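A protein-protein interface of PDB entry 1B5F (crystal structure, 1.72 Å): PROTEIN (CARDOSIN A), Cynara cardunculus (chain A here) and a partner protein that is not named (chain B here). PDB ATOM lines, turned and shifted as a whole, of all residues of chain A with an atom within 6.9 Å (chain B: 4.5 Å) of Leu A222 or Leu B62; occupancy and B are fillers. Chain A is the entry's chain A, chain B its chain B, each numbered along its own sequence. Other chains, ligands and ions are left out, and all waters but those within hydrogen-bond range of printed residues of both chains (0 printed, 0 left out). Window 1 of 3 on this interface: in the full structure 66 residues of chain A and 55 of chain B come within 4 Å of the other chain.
Among the printed residues, 37 pairs touch across the chains.
The side-chain carboxylate (OD1) of Asp A216 sits at hydrogen-bond distance from the backbone NH (N) of Gly A218, at 2.9 Å. O of Ala A215 is in hydrogen-bond range of OG1 of Thr A34 (2.8 Å). The backbone carbonyl oxygen (O) of Ala A213 is in hydrogen-bond range of the backbone NH (N) of Phe A192. The side-chain carboxylate of Asp A216 sits at hydrogen-bond distance from the side-chain hydroxyl of Thr A219 (2.6 Å). The side-chain hydroxyl of Thr A34 sits at hydrogen-bond distance from the backbone NH of Ser A217, 3.0 Å away.
Leu A222 touches ten residues of chain B. Leu B62 touches just these residues of chain A: Phe A214 (2.9 Å), Ala A215 (3.5 Å), Asp A216 (2.8 Å) and Leu A222 (3.8 Å). Of the printed residues of chain B, Leu A221 touches Gly B47, Thr B49, Ile B61, Gly B63 and Val B65. Of the printed residues of chain A, Ile B61 touches Phe A214 (3.7 Å), Asp A216 (3.6 Å), Thr A219 (3.9 Å), Leu A221 (3.8 Å), Leu A222 (3.3 Å) and Ser A223 (2.8 Å). The nearest printed residue of chain B that does not touch Leu A222 is Trp B60 (4.9 Å). The nearest residue of chain A that does not touch Leu B62 is Phe A192 (4.1 Å). The nearest printed residue of chain B that does not touch Asp A216 is Val B65 (6.8 Å).
CZ of Phe A214 touches CG1 of Ile B61, at 3.7 Å. O of Leu B62 touches CA of Ala A215, at 3.5 Å. Ile B61 touches Asp A216. Gly B63 touches Asp A216. CB of Leu A221 touches O of Gly B47, 3.3 Å away. Leu A221 touches Thr B49. O of Ile B61 touches O of Leu A221, 3.8 Å away. CD1 of Leu A222 touches CE1 of Phe B18 (3.9 Å). Leu A222 touches Ile B61 (CA to O, 3.3 Å). Trp B60 touches Ser A223 (CA to O, 3.1 Å).
The backbone carbonyl oxygen of Gly B47 sits at hydrogen-bond distance from the backbone NH of Leu A222 (2.9 Å). O of Leu B62 lies within hydrogen-bond range of N of Asp A216 (2.8 Å). The backbone NH (N) of Leu B62 is in hydrogen-bond range of the backbone carbonyl oxygen (O) of Phe A214, at 2.9 Å. N of Ile B61 sits at hydrogen-bond distance from O of Ser A223, 2.8 Å away. The side-chain hydroxyl (OG) of Ser A223 is in hydrogen-bond range of the side-chain hydroxyl (OG1) of Thr B49, at 3.1 Å. The backbone NH (N) of Gly B63 is in hydrogen-bond range of the backbone carbonyl oxygen (O) of Leu A221 (3.3 Å). The backbone carbonyl oxygen (O) of Ser A220 sits at hydrogen-bond distance from the backbone NH (N) of Val B65 (3.1 Å). SD of Met B67 sits at hydrogen-bond distance from N of Asp A216 (3.8 Å). N of Phe A214 sits at hydrogen-bond distance from O of Trp B60, 3.0 Å away. The backbone NH (N) of Ser A217 lies within hydrogen-bond range of the side-chain sulfur (SD) of Met B67 (3.6 Å). The backbone NH (N) of Thr B49 lies within hydrogen-bond range of the backbone carbonyl oxygen (O) of Leu A222, 2.8 Å away. The backbone NH (N) of Gly A224 lies within hydrogen-bond range of the backbone carbonyl oxygen (O) of Thr B49, 2.9 Å away.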
ATOM      1  N   THR A  34      -4.863   4.707 -13.406  1.00  0.00           N
ATOM      2  CA  THR A  34      -5.563   4.056 -12.334  1.00  0.00           C
ATOM      3  C   THR A  34      -6.937   3.615 -12.831  1.00  0.00           C
ATOM      4  O   THR A  34      -7.676   2.941 -12.121  1.00  0.00           O
ATOM      5  CB  THR A  34      -5.727   4.937 -11.078  1.00  0.00           C
ATOM      6  OG1 THR A  34      -6.301   6.190 -11.454  1.00  0.00           O
ATOM      7  CG2 THR A  34      -4.444   5.333 -10.397  1.00  0.00           C
ATOM      8  N   PHE A 192     -15.501   4.166  -5.365  1.00  0.00           N
ATOM      9  CA  PHE A 192     -15.999   4.467  -4.047  1.00  0.00           C
ATOM     10  C   PHE A 192     -17.350   5.162  -4.173  1.00  0.00           C
ATOM     11  O   PHE A 192     -17.717   5.588  -5.274  1.00  0.00           O
ATOM     12  CB  PHE A 192     -14.977   5.313  -3.283  1.00  0.00           C
ATOM     13  CG  PHE A 192     -14.515   6.514  -4.101  1.00  0.00           C
ATOM     14  CD1 PHE A 192     -15.233   7.698  -4.059  1.00  0.00           C
ATOM     15  CD2 PHE A 192     -13.393   6.429  -4.890  1.00  0.00           C
ATOM     16  CE1 PHE A 192     -14.836   8.795  -4.805  1.00  0.00           C
ATOM     17  CE2 PHE A 192     -12.997   7.510  -5.656  1.00  0.00           C
ATOM     18  CZ  PHE A 192     -13.734   8.673  -5.636  1.00  0.00           C
ATOM     19  N   ILE A 194     -20.136   8.176  -3.555  1.00  0.00           N
ATOM     20  CA  ILE A 194     -20.155   9.618  -3.347  1.00  0.00           C
ATOM     21  C   ILE A 194     -21.565  10.093  -3.016  1.00  0.00           C
ATOM     22  O   ILE A 194     -22.507   9.346  -3.233  1.00  0.00           O
ATOM     23  CB  ILE A 194     -19.663  10.394  -4.584  1.00  0.00           C
ATOM     24  CG1 ILE A 194     -20.534  10.226  -5.833  1.00  0.00           C
ATOM     25  CG2 ILE A 194     -18.217  10.045  -4.872  1.00  0.00           C
ATOM     26  CD1 ILE A 194     -20.255  11.293  -6.891  1.00  0.00           C
ATOM     27  N   ALA A 213     -18.125   6.700  -7.912  1.00  0.00           N
ATOM     28  CA  ALA A 213     -17.103   7.401  -8.662  1.00  0.00           C
ATOM     29  C   ALA A 213     -15.798   6.623  -8.606  1.00  0.00           C
ATOM     30  O   ALA A 213     -15.590   5.891  -7.643  1.00  0.00           O
ATOM     31  CB  ALA A 213     -16.892   8.800  -8.100  1.00  0.00           C
ATOM     32  N   PHE A 214     -14.963   6.824  -9.617  1.00  0.00           N
ATOM     33  CA  PHE A 214     -13.605   6.316  -9.503  1.00  0.00           C
ATOM     34  C   PHE A 214     -12.632   7.415  -9.917  1.00  0.00           C
ATOM     35  O   PHE A 214     -12.976   8.260 -10.732  1.00  0.00           O
ATOM     36  CB  PHE A 214     -13.355   5.051 -10.283  1.00  0.00           C
ATOM     37  CG  PHE A 214     -13.520   4.986 -11.785  1.00  0.00           C
ATOM     38  CD1 PHE A 214     -14.745   4.734 -12.374  1.00  0.00           C
ATOM     39  CD2 PHE A 214     -12.435   5.141 -12.618  1.00  0.00           C
ATOM     40  CE1 PHE A 214     -14.886   4.642 -13.752  1.00  0.00           C
ATOM     41  CE2 PHE A 214     -12.557   5.064 -13.996  1.00  0.00           C
ATOM     42  CZ  PHE A 214     -13.794   4.803 -14.573  1.00  0.00           C
ATOM     43  N   ALA A 215     -11.461   7.353  -9.297  1.00  0.00           N
ATOM     44  CA  ALA A 215     -10.370   8.285  -9.569  1.00  0.00           C
ATOM     45  C   ALA A 215      -9.505   7.743 -10.700  1.00  0.00           C
ATOM     46  O   ALA A 215      -8.957   6.663 -10.564  1.00  0.00           O
ATOM     47  CB  ALA A 215      -9.571   8.546  -8.299  1.00  0.00           C
ATOM     48  N   ASP A 216      -9.395   8.502 -11.785  1.00  0.00           N
ATOM     49  CA  ASP A 216      -8.815   8.039 -13.045  1.00  0.00           C
ATOM     50  C   ASP A 216      -7.733   8.985 -13.531  1.00  0.00           C
ATOM     51  O   ASP A 216      -7.976   9.974 -14.210  1.00  0.00           O
ATOM     52  CB  ASP A 216      -9.878   7.841 -14.115  1.00  0.00           C
ATOM     53  CG  ASP A 216      -9.312   7.190 -15.366  1.00  0.00           C
ATOM     54  OD1 ASP A 216      -8.096   6.951 -15.413  1.00  0.00           O
ATOM     55  OD2 ASP A 216     -10.100   6.940 -16.291  1.00  0.00           O
ATOM     56  N   SER A 217      -6.479   8.684 -13.192  1.00  0.00           N
ATOM     57  CA  SER A 217      -5.444   9.639 -13.578  1.00  0.00           C
ATOM     58  C   SER A 217      -5.200   9.623 -15.077  1.00  0.00           C
ATOM     59  O   SER A 217      -4.542  10.535 -15.594  1.00  0.00           O
ATOM     60  CB  SER A 217      -4.169   9.307 -12.829  1.00  0.00           C
ATOM     61  OG  SER A 217      -3.648   8.090 -13.347  1.00  0.00           O
ATOM     62  N   GLY A 218      -5.734   8.583 -15.731  1.00  0.00           N
ATOM     63  CA  GLY A 218      -5.550   8.479 -17.173  1.00  0.00           C
ATOM     64  C   GLY A 218      -6.631   9.118 -18.009  1.00  0.00           C
ATOM     65  O   GLY A 218      -6.685   8.909 -19.230  1.00  0.00           O
ATOM     66  N   THR A 219      -7.525   9.883 -17.414  1.00  0.00           N
ATOM     67  CA  THR A 219      -8.659  10.557 -18.009  1.00  0.00           C
ATOM     68  C   THR A 219      -8.476  12.060 -17.751  1.00  0.00           C
ATOM     69  O   THR A 219      -8.048  12.456 -16.655  1.00  0.00           O
ATOM     70  CB  THR A 219     -10.001  10.090 -17.389  1.00  0.00           C
ATOM     71  OG1 THR A 219     -10.476   8.883 -17.994  1.00  0.00           O
ATOM     72  CG2 THR A 219     -11.130  11.087 -17.594  1.00  0.00           C
ATOM     73  N   SER A 220      -8.793  12.885 -18.729  1.00  0.00           N
ATOM     74  CA  SER A 220      -8.599  14.318 -18.680  1.00  0.00           C
ATOM     75  C   SER A 220      -9.621  15.061 -17.838  1.00  0.00           C
ATOM     76  O   SER A 220      -9.267  15.881 -16.991  1.00  0.00           O
ATOM     77  CB  SER A 220      -8.711  14.922 -20.103  1.00  0.00           C
ATOM     78  OG  SER A 220      -8.673  16.334 -19.919  1.00  0.00           O
ATOM     79  N   LEU A 221     -10.899  14.794 -18.115  1.00  0.00           N
ATOM     80  CA  LEU A 221     -11.985  15.593 -17.559  1.00  0.00           C
ATOM     81  C   LEU A 221     -12.767  14.802 -16.520  1.00  0.00           C
ATOM     82  O   LEU A 221     -12.353  13.719 -16.113  1.00  0.00           O
ATOM     83  CB  LEU A 221     -12.901  16.079 -18.689  1.00  0.00           C
ATOM     84  CG  LEU A 221     -12.179  16.801 -19.839  1.00  0.00           C
ATOM     85  CD1 LEU A 221     -13.188  17.204 -20.896  1.00  0.00           C
ATOM     86  CD2 LEU A 221     -11.406  17.981 -19.282  1.00  0.00           C
ATOM     87  N   LEU A 222     -13.868  15.360 -16.080  1.00  0.00           N
ATOM     88  CA  LEU A 222     -14.830  14.742 -15.200  1.00  0.00           C
ATOM     89  C   LEU A 222     -16.011  14.239 -16.018  1.00  0.00           C
ATOM     90  O   LEU A 222     -16.591  15.022 -16.769  1.00  0.00           O
ATOM     91  CB  LEU A 222     -15.376  15.748 -14.188  1.00  0.00           C
ATOM     92  CG  LEU A 222     -14.345  16.474 -13.344  1.00  0.00           C
ATOM     93  CD1 LEU A 222     -15.008  17.321 -12.259  1.00  0.00           C
ATOM     94  CD2 LEU A 222     -13.407  15.459 -12.717  1.00  0.00           C
ATOM     95  N   SER A 223     -16.366  12.985 -15.878  1.00  0.00           N
ATOM     96  CA  SER A 223     -17.515  12.464 -16.610  1.00  0.00           C
ATOM     97  C   SER A 223     -18.587  12.053 -15.631  1.00  0.00           C
ATOM     98  O   SER A 223     -18.248  11.457 -14.612  1.00  0.00           O
ATOM     99  CB  SER A 223     -17.108  11.237 -17.458  1.00  0.00           C
ATOM    100  OG  SER A 223     -16.088  11.623 -18.350  1.00  0.00           O
ATOM    101  N   GLY A 224     -19.845  12.363 -15.919  1.00  0.00           N
ATOM    102  CA  GLY A 224     -20.870  11.950 -14.978  1.00  0.00           C
ATOM    103  C   GLY A 224     -22.253  11.941 -15.620  1.00  0.00           C
ATOM    104  O   GLY A 224     -22.374  12.314 -16.786  1.00  0.00           O
ATOM    105  N   VAL A 229     -24.752  16.673 -15.100  1.00  0.00           N
ATOM    106  CA  VAL A 229     -23.846  17.487 -15.893  1.00  0.00           C
ATOM    107  C   VAL A 229     -24.604  18.513 -16.716  1.00  0.00           C
ATOM    108  O   VAL A 229     -24.105  19.621 -16.942  1.00  0.00           O
ATOM    109  CB  VAL A 229     -22.964  16.619 -16.798  1.00  0.00           C
ATOM    110  CG1 VAL A 229     -22.192  17.489 -17.782  1.00  0.00           C
ATOM    111  CG2 VAL A 229     -22.025  15.755 -15.946  1.00  0.00           C
ATOM    112  N   PHE B  18     -18.356  18.023  -4.849  1.00  0.00           N
ATOM    113  CA  PHE B  18     -18.638  16.613  -4.688  1.00  0.00           C
ATOM    114  C   PHE B  18     -18.579  16.226  -3.211  1.00  0.00           C
ATOM    115  O   PHE B  18     -17.592  16.546  -2.559  1.00  0.00           O
ATOM    116  CB  PHE B  18     -17.619  15.749  -5.448  1.00  0.00           C
ATOM    117  CG  PHE B  18     -17.746  15.902  -6.960  1.00  0.00           C
ATOM    118  CD1 PHE B  18     -17.078  16.921  -7.618  1.00  0.00           C
ATOM    119  CD2 PHE B  18     -18.531  15.008  -7.686  1.00  0.00           C
ATOM    120  CE1 PHE B  18     -17.165  17.088  -8.987  1.00  0.00           C
ATOM    121  CE2 PHE B  18     -18.624  15.192  -9.057  1.00  0.00           C
ATOM    122  CZ  PHE B  18     -17.951  16.199  -9.705  1.00  0.00           C
ATOM    123  N   ILE B  20     -17.868  13.480  -0.613  1.00  0.00           N
ATOM    124  CA  ILE B  20     -17.096  12.259  -0.485  1.00  0.00           C
ATOM    125  C   ILE B  20     -16.733  12.014   0.978  1.00  0.00           C
ATOM    126  O   ILE B  20     -16.154  12.856   1.665  1.00  0.00           O
ATOM    127  CB  ILE B  20     -15.808  12.296  -1.327  1.00  0.00           C
ATOM    128  CG1 ILE B  20     -16.020  12.740  -2.773  1.00  0.00           C
ATOM    129  CG2 ILE B  20     -15.074  10.955  -1.317  1.00  0.00           C
ATOM    130  CD1 ILE B  20     -14.741  12.894  -3.574  1.00  0.00           C
ATOM    131  N   LEU B  27     -14.621  22.364  -6.333  1.00  0.00           N
ATOM    132  CA  LEU B  27     -13.795  22.800  -7.456  1.00  0.00           C
ATOM    133  C   LEU B  27     -14.127  24.240  -7.838  1.00  0.00           C
ATOM    134  O   LEU B  27     -15.305  24.550  -7.998  1.00  0.00           O
ATOM    135  CB  LEU B  27     -14.018  21.893  -8.663  1.00  0.00           C
ATOM    136  CG  LEU B  27     -13.726  20.411  -8.463  1.00  0.00           C
ATOM    137  CD1 LEU B  27     -14.245  19.574  -9.642  1.00  0.00           C
ATOM    138  CD2 LEU B  27     -12.231  20.182  -8.318  1.00  0.00           C
ATOM    139  N   GLY B  47     -14.888  21.310 -18.016  1.00  0.00           N
ATOM    140  CA  GLY B  47     -14.283  20.055 -17.591  1.00  0.00           C
ATOM    141  C   GLY B  47     -15.307  19.006 -17.228  1.00  0.00           C
ATOM    142  O   GLY B  47     -14.998  17.887 -16.813  1.00  0.00           O
ATOM    143  N   PHE B  48     -16.578  19.347 -17.384  1.00  0.00           N
ATOM    144  CA  PHE B  48     -17.631  18.400 -17.076  1.00  0.00           C
ATOM    145  C   PHE B  48     -18.231  17.821 -18.364  1.00  0.00           C
ATOM    146  O   PHE B  48     -18.778  18.570 -19.185  1.00  0.00           O
ATOM    147  CB  PHE B  48     -18.760  19.026 -16.275  1.00  0.00           C
ATOM    148  CG  PHE B  48     -18.346  19.646 -14.957  1.00  0.00           C
ATOM    149  CD1 PHE B  48     -18.346  18.863 -13.815  1.00  0.00           C
ATOM    150  CD2 PHE B  48     -17.967  20.971 -14.888  1.00  0.00           C
ATOM    151  CE1 PHE B  48     -17.953  19.410 -12.603  1.00  0.00           C
ATOM    152  CE2 PHE B  48     -17.570  21.512 -13.683  1.00  0.00           C
ATOM    153  CZ  PHE B  48     -17.557  20.725 -12.554  1.00  0.00           C
ATOM    154  N   THR B  49     -18.142  16.509 -18.520  1.00  0.00           N
ATOM    155  CA  THR B  49     -18.716  15.841 -19.692  1.00  0.00           C
ATOM    156  C   THR B  49     -19.707  14.784 -19.228  1.00  0.00           C
ATOM    157  O   THR B  49     -19.610  14.225 -18.141  1.00  0.00           O
ATOM    158  CB  THR B  49     -17.670  15.184 -20.597  1.00  0.00           C
ATOM    159  OG1 THR B  49     -16.954  14.256 -19.779  1.00  0.00           O
ATOM    160  CG2 THR B  49     -16.659  16.166 -21.131  1.00  0.00           C
ATOM    161  N   TRP B  60     -19.538   8.303 -11.919  1.00  0.00           N
ATOM    162  CA  TRP B  60     -18.696   9.420 -12.253  1.00  0.00           C
ATOM    163  C   TRP B  60     -17.238   8.973 -12.442  1.00  0.00           C
ATOM    164  O   TRP B  60     -16.722   8.124 -11.710  1.00  0.00           O
ATOM    165  CB  TRP B  60     -18.682  10.473 -11.147  1.00  0.00           C
ATOM    166  CG  TRP B  60     -19.932  11.248 -10.933  1.00  0.00           C
ATOM    167  CD1 TRP B  60     -21.045  10.886 -10.239  1.00  0.00           C
ATOM    168  CD2 TRP B  60     -20.170  12.566 -11.460  1.00  0.00           C
ATOM    169  NE1 TRP B  60     -21.969  11.911 -10.298  1.00  0.00           N
ATOM    170  CE2 TRP B  60     -21.456  12.941 -11.036  1.00  0.00           C
ATOM    171  CE3 TRP B  60     -19.379  13.417 -12.243  1.00  0.00           C
ATOM    172  CZ2 TRP B  60     -21.983  14.180 -11.386  1.00  0.00           C
ATOM    173  CZ3 TRP B  60     -19.912  14.657 -12.590  1.00  0.00           C
ATOM    174  CH2 TRP B  60     -21.193  14.999 -12.155  1.00  0.00           C
ATOM    175  N   ILE B  61     -16.559   9.575 -13.412  1.00  0.00           N
ATOM    176  CA  ILE B  61     -15.131   9.428 -13.589  1.00  0.00           C
ATOM    177  C   ILE B  61     -14.468  10.744 -13.173  1.00  0.00           C
ATOM    178  O   ILE B  61     -14.733  11.747 -13.818  1.00  0.00           O
ATOM    179  CB  ILE B  61     -14.726   9.116 -15.029  1.00  0.00           C
ATOM    180  CG1 ILE B  61     -15.511   7.951 -15.640  1.00  0.00           C
ATOM    181  CG2 ILE B  61     -13.229   8.876 -15.090  1.00  0.00           C
ATOM    182  CD1 ILE B  61     -15.266   7.760 -17.124  1.00  0.00           C
ATOM    183  N   LEU B  62     -13.669  10.695 -12.127  1.00  0.00           N
ATOM    184  CA  LEU B  62     -12.925  11.820 -11.586  1.00  0.00           C
ATOM    185  C   LEU B  62     -11.495  11.726 -12.123  1.00  0.00           C
ATOM    186  O   LEU B  62     -10.592  11.078 -11.604  1.00  0.00           O
ATOM    187  CB  LEU B  62     -12.960  11.872 -10.065  1.00  0.00           C
ATOM    188  CG  LEU B  62     -14.331  11.909  -9.398  1.00  0.00           C
ATOM    189  CD1 LEU B  62     -14.215  12.048  -7.881  1.00  0.00           C
ATOM    190  CD2 LEU B  62     -15.192  13.032  -9.964  1.00  0.00           C
ATOM    191  N   GLY B  63     -11.308  12.411 -13.249  1.00  0.00           N
ATOM    192  CA  GLY B  63     -10.081  12.472 -13.988  1.00  0.00           C
ATOM    193  C   GLY B  63      -9.184  13.590 -13.527  1.00  0.00           C
ATOM    194  O   GLY B  63      -9.281  14.063 -12.381  1.00  0.00           O
ATOM    195  N   VAL B  65      -8.999  16.658 -13.957  1.00  0.00           N
ATOM    196  CA  VAL B  65      -9.598  17.903 -13.464  1.00  0.00           C
ATOM    197  C   VAL B  65      -9.707  17.883 -11.945  1.00  0.00           C
ATOM    198  O   VAL B  65      -9.463  18.888 -11.284  1.00  0.00           O
ATOM    199  CB  VAL B  65     -10.975  18.122 -14.094  1.00  0.00           C
ATOM    200  CG1 VAL B  65     -11.821  19.116 -13.305  1.00  0.00           C
ATOM    201  CG2 VAL B  65     -10.860  18.636 -15.529  1.00  0.00           C
ATOM    202  N   PHE B  66     -10.085  16.736 -11.387  1.00  0.00           N
ATOM    203  CA  PHE B  66     -10.259  16.565  -9.952  1.00  0.00           C
ATOM    204  C   PHE B  66      -8.951  16.238  -9.243  1.00  0.00           C
ATOM    205  O   PHE B  66      -8.731  16.710  -8.124  1.00  0.00           O
ATOM    206  CB  PHE B  66     -11.234  15.426  -9.677  1.00  0.00           C
ATOM    207  CG  PHE B  66     -11.658  15.307  -8.236  1.00  0.00           C
ATOM    208  CD1 PHE B  66     -12.773  16.014  -7.809  1.00  0.00           C
ATOM    209  CD2 PHE B  66     -10.989  14.515  -7.323  1.00  0.00           C
ATOM    210  CE1 PHE B  66     -13.198  15.929  -6.496  1.00  0.00           C
ATOM    211  CE2 PHE B  66     -11.398  14.453  -6.007  1.00  0.00           C
ATOM    212  CZ  PHE B  66     -12.499  15.159  -5.586  1.00  0.00           C
ATOM    213  N   MET B  67      -8.128  15.409  -9.875  1.00  0.00           N
ATOM    214  CA  MET B  67      -6.877  14.948  -9.290  1.00  0.00           C
ATOM    215  C   MET B  67      -5.759  15.978  -9.279  1.00  0.00           C
ATOM    216  O   MET B  67      -4.706  15.750  -8.658  1.00  0.00           O
ATOM    217  CB  MET B  67      -6.419  13.646 -10.018  1.00  0.00           C
ATOM    218  CG  MET B  67      -7.415  12.530  -9.696  1.00  0.00           C
ATOM    219  SD  MET B  67      -6.878  10.940 -10.378  1.00  0.00           S
ATOM    220  CE  MET B  67      -5.383  10.634  -9.443  1.00  0.00           C
